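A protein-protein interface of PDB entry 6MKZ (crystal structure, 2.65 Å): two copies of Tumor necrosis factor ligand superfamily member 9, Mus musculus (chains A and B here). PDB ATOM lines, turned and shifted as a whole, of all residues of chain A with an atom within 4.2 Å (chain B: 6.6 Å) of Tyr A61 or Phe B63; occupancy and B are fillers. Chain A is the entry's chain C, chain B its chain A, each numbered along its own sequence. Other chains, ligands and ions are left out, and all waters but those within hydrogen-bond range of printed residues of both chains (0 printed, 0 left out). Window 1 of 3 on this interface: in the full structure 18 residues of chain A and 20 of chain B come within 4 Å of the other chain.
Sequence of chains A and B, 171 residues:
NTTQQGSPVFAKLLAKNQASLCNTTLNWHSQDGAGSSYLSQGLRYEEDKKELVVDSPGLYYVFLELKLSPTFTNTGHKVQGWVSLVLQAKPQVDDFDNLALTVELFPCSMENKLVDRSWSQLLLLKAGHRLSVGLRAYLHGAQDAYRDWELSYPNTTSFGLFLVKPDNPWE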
ATOM      1  N   TYR A  60       4.807  -7.252 -29.522  1.00  0.00           N
ATOM      2  CA  TYR A  60       4.453  -8.665 -29.473  1.00  0.00           C
ATOM      3  C   TYR A  60       5.636  -9.534 -29.159  1.00  0.00           C
ATOM      4  O   TYR A  60       6.695  -9.362 -29.751  1.00  0.00           O
ATOM      5  CB  TYR A  60       3.868  -9.110 -30.821  1.00  0.00           C
ATOM      6  CG  TYR A  60       2.428  -8.714 -31.027  1.00  0.00           C
ATOM      7  CD1 TYR A  60       2.095  -7.456 -31.528  1.00  0.00           C
ATOM      8  CD2 TYR A  60       1.393  -9.587 -30.717  1.00  0.00           C
ATOM      9  CE1 TYR A  60       0.768  -7.090 -31.739  1.00  0.00           C
ATOM     10  CE2 TYR A  60       0.061  -9.225 -30.906  1.00  0.00           C
ATOM     11  CZ  TYR A  60      -0.249  -7.968 -31.405  1.00  0.00           C
ATOM     12  OH  TYR A  60      -1.566  -7.614 -31.598  1.00  0.00           O
ATOM     13  N   TYR A  61       5.453 -10.486 -28.248  1.00  0.00           N
ATOM     14  CA  TYR A  61       6.456 -11.497 -27.932  1.00  0.00           C
ATOM     15  C   TYR A  61       6.191 -12.657 -28.865  1.00  0.00           C
ATOM     16  O   TYR A  61       5.216 -13.387 -28.651  1.00  0.00           O
ATOM     17  CB  TYR A  61       6.366 -11.905 -26.456  1.00  0.00           C
ATOM     18  CG  TYR A  61       7.310 -13.006 -26.042  1.00  0.00           C
ATOM     19  CD1 TYR A  61       8.632 -12.726 -25.700  1.00  0.00           C
ATOM     20  CD2 TYR A  61       6.863 -14.314 -25.899  1.00  0.00           C
ATOM     21  CE1 TYR A  61       9.489 -13.726 -25.247  1.00  0.00           C
ATOM     22  CE2 TYR A  61       7.716 -15.328 -25.467  1.00  0.00           C
ATOM     23  CZ  TYR A  61       9.025 -15.029 -25.130  1.00  0.00           C
ATOM     24  OH  TYR A  61       9.867 -16.036 -24.711  1.00  0.00           O
ATOM     25  N   VAL A  62       6.967 -12.758 -29.961  1.00  0.00           N
ATOM     26  CA  VAL A  62       6.779 -13.806 -30.976  1.00  0.00           C
ATOM     27  C   VAL A  62       7.735 -14.959 -30.689  1.00  0.00           C
ATOM     28  O   VAL A  62       8.898 -14.705 -30.380  1.00  0.00           O
ATOM     29  CB  VAL A  62       6.923 -13.273 -32.429  1.00  0.00           C
ATOM     30  CG1 VAL A  62       6.596 -14.368 -33.449  1.00  0.00           C
ATOM     31  CG2 VAL A  62       6.020 -12.061 -32.653  1.00  0.00           C
ATOM     32  N   PHE A  63       7.248 -16.217 -30.769  1.00  0.00           N
ATOM     33  CA  PHE A  63       8.074 -17.388 -30.485  1.00  0.00           C
ATOM     34  C   PHE A  63       7.851 -18.498 -31.504  1.00  0.00           C
ATOM     35  O   PHE A  63       6.765 -18.636 -32.070  1.00  0.00           O
ATOM     36  CB  PHE A  63       7.862 -17.927 -29.051  1.00  0.00           C
ATOM     37  CG  PHE A  63       6.432 -18.274 -28.692  1.00  0.00           C
ATOM     38  CD1 PHE A  63       5.919 -19.551 -28.945  1.00  0.00           C
ATOM     39  CD2 PHE A  63       5.595 -17.330 -28.114  1.00  0.00           C
ATOM     40  CE1 PHE A  63       4.588 -19.860 -28.647  1.00  0.00           C
ATOM     41  CE2 PHE A  63       4.263 -17.644 -27.814  1.00  0.00           C
ATOM     42  CZ  PHE A  63       3.775 -18.910 -28.067  1.00  0.00           C
ATOM     43  N   SER A 120      12.616 -16.691 -29.608  1.00  0.00           N
ATOM     44  CA  SER A 120      11.653 -15.697 -29.117  1.00  0.00           C
ATOM     45  C   SER A 120      12.178 -14.308 -29.364  1.00  0.00           C
ATOM     46  O   SER A 120      13.390 -14.063 -29.243  1.00  0.00           O
ATOM     47  CB  SER A 120      11.334 -15.905 -27.641  1.00  0.00           C
ATOM     48  OG  SER A 120      12.475 -15.763 -26.807  1.00  0.00           O
ATOM     49  N   GLN A 121      11.271 -13.394 -29.730  1.00  0.00           N
ATOM     50  CA  GLN A 121      11.645 -12.011 -30.020  1.00  0.00           C
ATOM     51  C   GLN A 121      10.500 -11.044 -29.764  1.00  0.00           C
ATOM     52  O   GLN A 121       9.386 -11.286 -30.217  1.00  0.00           O
ATOM     53  CB  GLN A 121      12.111 -11.896 -31.490  1.00  0.00           C
ATOM     54  CG  GLN A 121      13.013 -10.694 -31.796  1.00  0.00           C
ATOM     55  CD  GLN A 121      14.422 -10.866 -31.300  1.00  0.00           C
ATOM     56  OE1 GLN A 121      15.069 -11.908 -31.493  1.00  0.00           O
ATOM     57  NE2 GLN A 121      14.932  -9.830 -30.660  1.00  0.00           N
ATOM     58  N   LEU A 122      10.800  -9.921 -29.070  1.00  0.00           N
ATOM     59  CA  LEU A 122       9.853  -8.829 -28.812  1.00  0.00           C
ATOM     60  C   LEU A 122       9.886  -7.930 -30.033  1.00  0.00           C
ATOM     61  O   LEU A 122      10.932  -7.377 -30.355  1.00  0.00           O
ATOM     62  CB  LEU A 122      10.192  -8.071 -27.519  1.00  0.00           C
ATOM     63  CG  LEU A 122       9.815  -8.779 -26.213  1.00  0.00           C
ATOM     64  CD1 LEU A 122      10.501  -8.139 -25.039  1.00  0.00           C
ATOM     65  CD2 LEU A 122       8.323  -8.751 -25.970  1.00  0.00           C
ATOM     66  N   LEU A 161       2.487 -16.074 -30.564  1.00  0.00           N
ATOM     67  CA  LEU A 161       2.755 -14.720 -30.112  1.00  0.00           C
ATOM     68  C   LEU A 161       1.782 -14.315 -29.015  1.00  0.00           C
ATOM     69  O   LEU A 161       0.774 -14.979 -28.795  1.00  0.00           O
ATOM     70  CB  LEU A 161       2.739 -13.693 -31.269  1.00  0.00           C
ATOM     71  CG  LEU A 161       1.609 -13.757 -32.303  1.00  0.00           C
ATOM     72  CD1 LEU A 161       0.312 -13.255 -31.739  1.00  0.00           C
ATOM     73  CD2 LEU A 161       1.970 -12.933 -33.511  1.00  0.00           C
ATOM     74  N   PHE A 162       2.136 -13.240 -28.310  1.00  0.00           N
ATOM     75  CA  PHE A 162       1.407 -12.624 -27.221  1.00  0.00           C
ATOM     76  C   PHE A 162       1.621 -11.109 -27.323  1.00  0.00           C
ATOM     77  O   PHE A 162       2.708 -10.697 -27.721  1.00  0.00           O
ATOM     78  CB  PHE A 162       1.908 -13.183 -25.873  1.00  0.00           C
ATOM     79  CG  PHE A 162       1.140 -12.702 -24.663  1.00  0.00           C
ATOM     80  CD1 PHE A 162      -0.110 -13.231 -24.353  1.00  0.00           C
ATOM     81  CD2 PHE A 162       1.655 -11.709 -23.840  1.00  0.00           C
ATOM     82  CE1 PHE A 162      -0.814 -12.788 -23.227  1.00  0.00           C
ATOM     83  CE2 PHE A 162       0.924 -11.234 -22.741  1.00  0.00           C
ATOM     84  CZ  PHE A 162      -0.290 -11.789 -22.431  1.00  0.00           C
ATOM     85  N   VAL A 164       2.382  -7.984 -25.532  1.00  0.00           N
ATOM     86  CA  VAL A 164       3.025  -7.593 -24.268  1.00  0.00           C
ATOM     87  C   VAL A 164       2.658  -6.139 -23.887  1.00  0.00           C
ATOM     88  O   VAL A 164       2.395  -5.851 -22.712  1.00  0.00           O
ATOM     89  CB  VAL A 164       4.556  -7.808 -24.360  1.00  0.00           C
ATOM     90  CG1 VAL A 164       5.284  -7.195 -23.174  1.00  0.00           C
ATOM     91  CG2 VAL A 164       4.865  -9.291 -24.448  1.00  0.00           C
ATOM     92  N   PHE B  10       3.104 -10.067 -18.389  1.00  0.00           N
ATOM     93  CA  PHE B  10       4.180 -10.819 -19.011  1.00  0.00           C
ATOM     94  C   PHE B  10       5.492 -10.680 -18.260  1.00  0.00           C
ATOM     95  O   PHE B  10       5.826  -9.594 -17.807  1.00  0.00           O
ATOM     96  CB  PHE B  10       4.368 -10.346 -20.479  1.00  0.00           C
ATOM     97  CG  PHE B  10       5.617 -10.873 -21.169  1.00  0.00           C
ATOM     98  CD1 PHE B  10       5.732 -12.210 -21.512  1.00  0.00           C
ATOM     99  CD2 PHE B  10       6.686 -10.032 -21.449  1.00  0.00           C
ATOM    100  CE1 PHE B  10       6.895 -12.693 -22.127  1.00  0.00           C
ATOM    101  CE2 PHE B  10       7.841 -10.513 -22.073  1.00  0.00           C
ATOM    102  CZ  PHE B  10       7.940 -11.837 -22.398  1.00  0.00           C
ATOM    103  N   ALA B  11       6.278 -11.762 -18.208  1.00  0.00           N
ATOM    104  CA  ALA B  11       7.621 -11.782 -17.606  1.00  0.00           C
ATOM    105  C   ALA B  11       8.535 -12.712 -18.373  1.00  0.00           C
ATOM    106  O   ALA B  11       8.095 -13.749 -18.867  1.00  0.00           O
ATOM    107  CB  ALA B  11       7.564 -12.212 -16.148  1.00  0.00           C
ATOM    108  N   LYS B  12       9.786 -12.311 -18.508  1.00  0.00           N
ATOM    109  CA  LYS B  12      10.854 -13.104 -19.101  1.00  0.00           C
ATOM    110  C   LYS B  12      12.079 -12.763 -18.304  1.00  0.00           C
ATOM    111  O   LYS B  12      12.601 -11.650 -18.416  1.00  0.00           O
ATOM    112  CB  LYS B  12      11.028 -12.869 -20.613  1.00  0.00           C
ATOM    113  CG  LYS B  12      12.288 -13.524 -21.193  1.00  0.00           C
ATOM    114  CD  LYS B  12      11.961 -14.658 -22.123  1.00  0.00           C
ATOM    115  CE  LYS B  12      13.189 -15.204 -22.822  1.00  0.00           C
ATOM    116  NZ  LYS B  12      12.836 -16.050 -24.011  1.00  0.00           N
ATOM    117  N   LEU B  13      12.454 -13.671 -17.406  1.00  0.00           N
ATOM    118  CA  LEU B  13      13.595 -13.522 -16.516  1.00  0.00           C
ATOM    119  C   LEU B  13      14.759 -14.343 -17.037  1.00  0.00           C
ATOM    120  O   LEU B  13      14.548 -15.367 -17.691  1.00  0.00           O
ATOM    121  CB  LEU B  13      13.233 -13.958 -15.086  1.00  0.00           C
ATOM    122  CG  LEU B  13      11.938 -13.421 -14.446  1.00  0.00           C
ATOM    123  CD1 LEU B  13      11.941 -13.679 -12.961  1.00  0.00           C
ATOM    124  CD2 LEU B  13      11.781 -11.911 -14.647  1.00  0.00           C
ATOM    125  N   TYR B  61       0.468 -19.009 -19.293  1.00  0.00           N
ATOM    126  CA  TYR B  61       1.339 -19.810 -20.161  1.00  0.00           C
ATOM    127  C   TYR B  61       2.735 -19.676 -19.587  1.00  0.00           C
ATOM    128  O   TYR B  61       3.342 -18.617 -19.743  1.00  0.00           O
ATOM    129  CB  TYR B  61       1.252 -19.331 -21.618  1.00  0.00           C
ATOM    130  CG  TYR B  61       2.183 -20.032 -22.582  1.00  0.00           C
ATOM    131  CD1 TYR B  61       1.835 -21.245 -23.164  1.00  0.00           C
ATOM    132  CD2 TYR B  61       3.383 -19.451 -22.967  1.00  0.00           C
ATOM    133  CE1 TYR B  61       2.657 -21.854 -24.111  1.00  0.00           C
ATOM    134  CE2 TYR B  61       4.213 -20.051 -23.907  1.00  0.00           C
ATOM    135  CZ  TYR B  61       3.834 -21.238 -24.494  1.00  0.00           C
ATOM    136  OH  TYR B  61       4.681 -21.811 -25.399  1.00  0.00           O
ATOM    137  N   VAL B  62       3.197 -20.687 -18.828  1.00  0.00           N
ATOM    138  CA  VAL B  62       4.509 -20.646 -18.163  1.00  0.00           C
ATOM    139  C   VAL B  62       5.537 -21.383 -19.033  1.00  0.00           C
ATOM    140  O   VAL B  62       5.228 -22.450 -19.554  1.00  0.00           O
ATOM    141  CB  VAL B  62       4.466 -21.186 -16.702  1.00  0.00           C
ATOM    142  CG1 VAL B  62       5.823 -21.014 -16.010  1.00  0.00           C
ATOM    143  CG2 VAL B  62       3.364 -20.494 -15.883  1.00  0.00           C
ATOM    144  N   PHE B  63       6.739 -20.801 -19.210  1.00  0.00           N
ATOM    145  CA  PHE B  63       7.787 -21.400 -20.039  1.00  0.00           C
ATOM    146  C   PHE B  63       9.161 -21.333 -19.381  1.00  0.00           C
ATOM    147  O   PHE B  63       9.446 -20.418 -18.617  1.00  0.00           O
ATOM    148  CB  PHE B  63       7.838 -20.784 -21.458  1.00  0.00           C
ATOM    149  CG  PHE B  63       8.017 -19.288 -21.506  1.00  0.00           C
ATOM    150  CD1 PHE B  63       9.288 -18.725 -21.515  1.00  0.00           C
ATOM    151  CD2 PHE B  63       6.915 -18.437 -21.527  1.00  0.00           C
ATOM    152  CE1 PHE B  63       9.452 -17.332 -21.525  1.00  0.00           C
ATOM    153  CE2 PHE B  63       7.080 -17.047 -21.538  1.00  0.00           C
ATOM    154  CZ  PHE B  63       8.344 -16.503 -21.555  1.00  0.00           C
ATOM    155  N   LEU B  64      10.000 -22.324 -19.689  1.00  0.00           N
ATOM    156  CA  LEU B  64      11.371 -22.510 -19.241  1.00  0.00           C
ATOM    157  C   LEU B  64      12.224 -22.850 -20.431  1.00  0.00           C
ATOM    158  O   LEU B  64      11.777 -23.591 -21.300  1.00  0.00           O
ATOM    159  CB  LEU B  64      11.455 -23.648 -18.213  1.00  0.00           C
ATOM    160  CG  LEU B  64      10.793 -23.443 -16.852  1.00  0.00           C
ATOM    161  CD1 LEU B  64      10.662 -24.770 -16.122  1.00  0.00           C
ATOM    162  CD2 LEU B  64      11.585 -22.500 -15.999  1.00  0.00           C
ATOM    163  N   GLU B  65      13.454 -22.335 -20.482  1.00  0.00           N
ATOM    164  CA  GLU B  65      14.380 -22.631 -21.572  1.00  0.00           C
ATOM    165  C   GLU B  65      15.743 -22.884 -20.979  1.00  0.00           C
ATOM    166  O   GLU B  65      16.292 -21.994 -20.350  1.00  0.00           O
ATOM    167  CB  GLU B  65      14.396 -21.501 -22.606  1.00  0.00           C
ATOM    168  CG  GLU B  65      15.087 -21.903 -23.901  1.00  0.00           C
ATOM    169  CD  GLU B  65      14.980 -20.965 -25.092  1.00  0.00           C
ATOM    170  OE1 GLU B  65      14.253 -19.941 -25.028  1.00  0.00           O
ATOM    171  OE2 GLU B  65      15.641 -21.271 -26.110  1.00  0.00           O
ATOM    172  N   LEU B  87       9.751 -26.348 -12.057  1.00  0.00           N
ATOM    173  CA  LEU B  87       8.882 -25.269 -11.610  1.00  0.00           C
ATOM    174  C   LEU B  87       8.358 -25.599 -10.202  1.00  0.00           C
ATOM    175  O   LEU B  87       7.821 -26.687  -9.964  1.00  0.00           O
ATOM    176  CB  LEU B  87       7.740 -25.036 -12.609  1.00  0.00           C
ATOM    177  CG  LEU B  87       7.010 -23.705 -12.515  1.00  0.00           C
ATOM    178  CD1 LEU B  87       7.910 -22.541 -12.900  1.00  0.00           C
ATOM    179  CD2 LEU B  87       5.802 -23.712 -13.398  1.00  0.00           C
ATOM    180  N   TRP B 119      10.444 -25.851 -22.441  1.00  0.00           N
ATOM    181  CA  TRP B 119       9.283 -26.387 -21.737  1.00  0.00           C
ATOM    182  C   TRP B 119       8.226 -25.302 -21.632  1.00  0.00           C
ATOM    183  O   TRP B 119       8.566 -24.170 -21.349  1.00  0.00           O
ATOM    184  CB  TRP B 119       9.714 -26.884 -20.349  1.00  0.00           C
ATOM    185  CG  TRP B 119       8.608 -27.361 -19.454  1.00  0.00           C
ATOM    186  CD1 TRP B 119       8.204 -28.650 -19.263  1.00  0.00           C
ATOM    187  CD2 TRP B 119       7.827 -26.559 -18.553  1.00  0.00           C
ATOM    188  NE1 TRP B 119       7.190 -28.696 -18.333  1.00  0.00           N
ATOM    189  CE2 TRP B 119       6.948 -27.428 -17.870  1.00  0.00           C
ATOM    190  CE3 TRP B 119       7.774 -25.181 -18.267  1.00  0.00           C
ATOM    191  CZ2 TRP B 119       6.043 -26.971 -16.906  1.00  0.00           C
ATOM    192  CZ3 TRP B 119       6.878 -24.731 -17.310  1.00  0.00           C
ATOM    193  CH2 TRP B 119       6.029 -25.622 -16.638  1.00  0.00           C
ATOM    194  N   SER B 120       6.961 -25.632 -21.869  1.00  0.00           N
ATOM    195  CA  SER B 120       5.841 -24.683 -21.756  1.00  0.00           C
ATOM    196  C   SER B 120       4.587 -25.393 -21.243  1.00  0.00           C
ATOM    197  O   SER B 120       4.330 -26.543 -21.604  1.00  0.00           O
ATOM    198  CB  SER B 120       5.565 -23.980 -23.079  1.00  0.00           C
ATOM    199  OG  SER B 120       5.209 -24.879 -24.113  1.00  0.00           O
ATOM    200  N   GLN B 121       3.812 -24.706 -20.393  1.00  0.00           N
ATOM    201  CA  GLN B 121       2.600 -25.271 -19.798  1.00  0.00           C
ATOM    202  C   GLN B 121       1.581 -24.201 -19.415  1.00  0.00           C
ATOM    203  O   GLN B 121       1.937 -23.213 -18.775  1.00  0.00           O
ATOM    204  CB  GLN B 121       2.968 -26.091 -18.542  1.00  0.00           C
ATOM    205  CG  GLN B 121       1.946 -27.150 -18.129  1.00  0.00           C
ATOM    206  CD  GLN B 121       1.965 -28.369 -19.021  1.00  0.00           C
ATOM    207  OE1 GLN B 121       3.025 -28.930 -19.349  1.00  0.00           O
ATOM    208  NE2 GLN B 121       0.781 -28.806 -19.426  1.00  0.00           N
ATOM    209  N   SER B 158      16.408 -19.147 -19.366  1.00  0.00           N
ATOM    210  CA  SER B 158      15.351 -18.179 -19.093  1.00  0.00           C
ATOM    211  C   SER B 158      14.102 -18.811 -18.563  1.00  0.00           C
ATOM    212  O   SER B 158      13.879 -20.008 -18.720  1.00  0.00           O
ATOM    213  CB  SER B 158      15.030 -17.358 -20.340  1.00  0.00           C
ATOM    214  OG  SER B 158      14.797 -18.204 -21.452  1.00  0.00           O
ATOM    215  N   PHE B 159      13.274 -17.977 -17.930  1.00  0.00           N
ATOM    216  CA  PHE B 159      12.020 -18.386 -17.321  1.00  0.00           C
ATOM    217  C   PHE B 159      11.033 -17.258 -17.409  1.00  0.00           C
ATOM    218  O   PHE B 159      11.342 -16.127 -17.037  1.00  0.00           O
ATOM    219  CB  PHE B 159      12.279 -18.795 -15.856  1.00  0.00           C
ATOM    220  CG  PHE B 159      11.199 -18.619 -14.810  1.00  0.00           C
ATOM    221  CD1 PHE B 159       9.979 -19.268 -14.931  1.00  0.00           C
ATOM    222  CD2 PHE B 159      11.453 -17.915 -13.638  1.00  0.00           C
ATOM    223  CE1 PHE B 159       9.000 -19.143 -13.933  1.00  0.00           C
ATOM    224  CE2 PHE B 159      10.488 -17.824 -12.626  1.00  0.00           C
ATOM    225  CZ  PHE B 159       9.261 -18.422 -12.790  1.00  0.00           C
ATOM    226  N   GLY B 160       9.834 -17.576 -17.854  1.00  0.00           N
ATOM    227  CA  GLY B 160       8.790 -16.568 -17.947  1.00  0.00           C
ATOM    228  C   GLY B 160       7.380 -17.104 -18.017  1.00  0.00           C
ATOM    229  O   GLY B 160       7.163 -18.313 -18.018  1.00  0.00           O
ATOM    230  N   LEU B 161       6.417 -16.179 -18.057  1.00  0.00           N
ATOM    231  CA  LEU B 161       4.991 -16.471 -18.141  1.00  0.00           C
ATOM    232  C   LEU B 161       4.230 -15.298 -18.739  1.00  0.00           C
ATOM    233  O   LEU B 161       4.772 -14.204 -18.861  1.00  0.00           O
ATOM    234  CB  LEU B 161       4.403 -16.854 -16.763  1.00  0.00           C
ATOM    235  CG  LEU B 161       4.761 -16.005 -15.533  1.00  0.00           C
ATOM    236  CD1 LEU B 161       4.059 -14.669 -15.552  1.00  0.00           C
ATOM    237  CD2 LEU B 161       4.347 -16.715 -14.271  1.00  0.00           C
ATOM    238  N   PHE B 162       2.973 -15.546 -19.123  1.00  0.00           N
ATOM    239  CA  PHE B 162       2.033 -14.539 -19.599  1.00  0.00           C
ATOM    240  C   PHE B 162       0.618 -14.984 -19.343  1.00  0.00           C
ATOM    241  O   PHE B 162       0.293 -16.165 -19.476  1.00  0.00           O
ATOM    242  CB  PHE B 162       2.225 -14.075 -21.047  1.00  0.00           C
ATOM    243  CG  PHE B 162       2.693 -15.027 -22.109  1.00  0.00           C
ATOM    244  CD1 PHE B 162       1.783 -15.679 -22.926  1.00  0.00           C
ATOM    245  CD2 PHE B 162       4.049 -15.173 -22.384  1.00  0.00           C
ATOM    246  CE1 PHE B 162       2.224 -16.513 -23.961  1.00  0.00           C
ATOM    247  CE2 PHE B 162       4.486 -15.994 -23.429  1.00  0.00           C
ATOM    248  CZ  PHE B 162       3.574 -16.645 -24.216  1.00  0.00           C
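Hydrophobic or aromatic side chains of chain B within 4 Å of the printed part of chain A: Phe B10, Tyr B61, Phe B63 and Phe B162.
The side-chain amino group (NZ) of Lys B12 lies within hydrogen-bond range of the side-chain hydroxyl (OG) of Ser A120 (2.8 Å). The side-chain hydroxyl (OH) of Tyr A61 is in hydrogen-bond range of the side-chain amino group (NZ) of Lys B12 (3.1 Å).
Tyr A61 touches Phe B63, and with the chains exchanged Phe A63 touches Tyr B61. Tyr A61 touches Phe B162, but with the chains exchanged Phe A162 does not touch Tyr B61 (6.8 Å). Phe A63 touches Phe B162, but with the chains exchanged Phe A162 does not touch Phe B63 (7.8 Å). Phe A162 touches its own counterpart, Phe B162. Positions printed for both chains: 61, 62, 63, 120, 121, 161 and 162.
The backbone NH (N) of Phe B63 sits at hydrogen-bond distance from the backbone carbonyl oxygen (O) of Gly B160 (2.8 Å). The side-chain hydroxyl (OH) of Tyr B61 lies close to the side-chain hydroxyl (OG) of Ser B120, at 3.4 Å. The side-chain hydroxyl of Tyr A61 lies close to the side-chain hydroxyl of Ser A120, at 3.4 Å. O of Phe B162 sits at hydrogen-bond distance from N of Tyr B61. The backbone NH (N) of Tyr A61 sits at hydrogen-bond distance from the backbone carbonyl oxygen (O) of Phe A162 (2.8 Å).
Tyr A61 touches Phe B10 (CD1 to CZ, 3.5 Å). Tyr A61 touches Phe B63. Tyr A61 touches Phe B162 (CD2 to CE2, 3.8 Å). OH of Tyr B61 touches CE1 of Phe A63, 3.8 Å away. Phe B162 touches Phe A63 (CZ to CE2, 3.8 Å). Phe B162 touches Phe A162. Val A164 touches Phe B10.
Of the printed residues of chain B, Val A164 touches Phe B10. Printed residues of chain A within 4 Å of Phe B10: Tyr A61 and Val A164. Phe B63 touches just one residue of chain A: Tyr A61 (3.5 Å). Leu B64 touches none of the printed residues of chain A.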
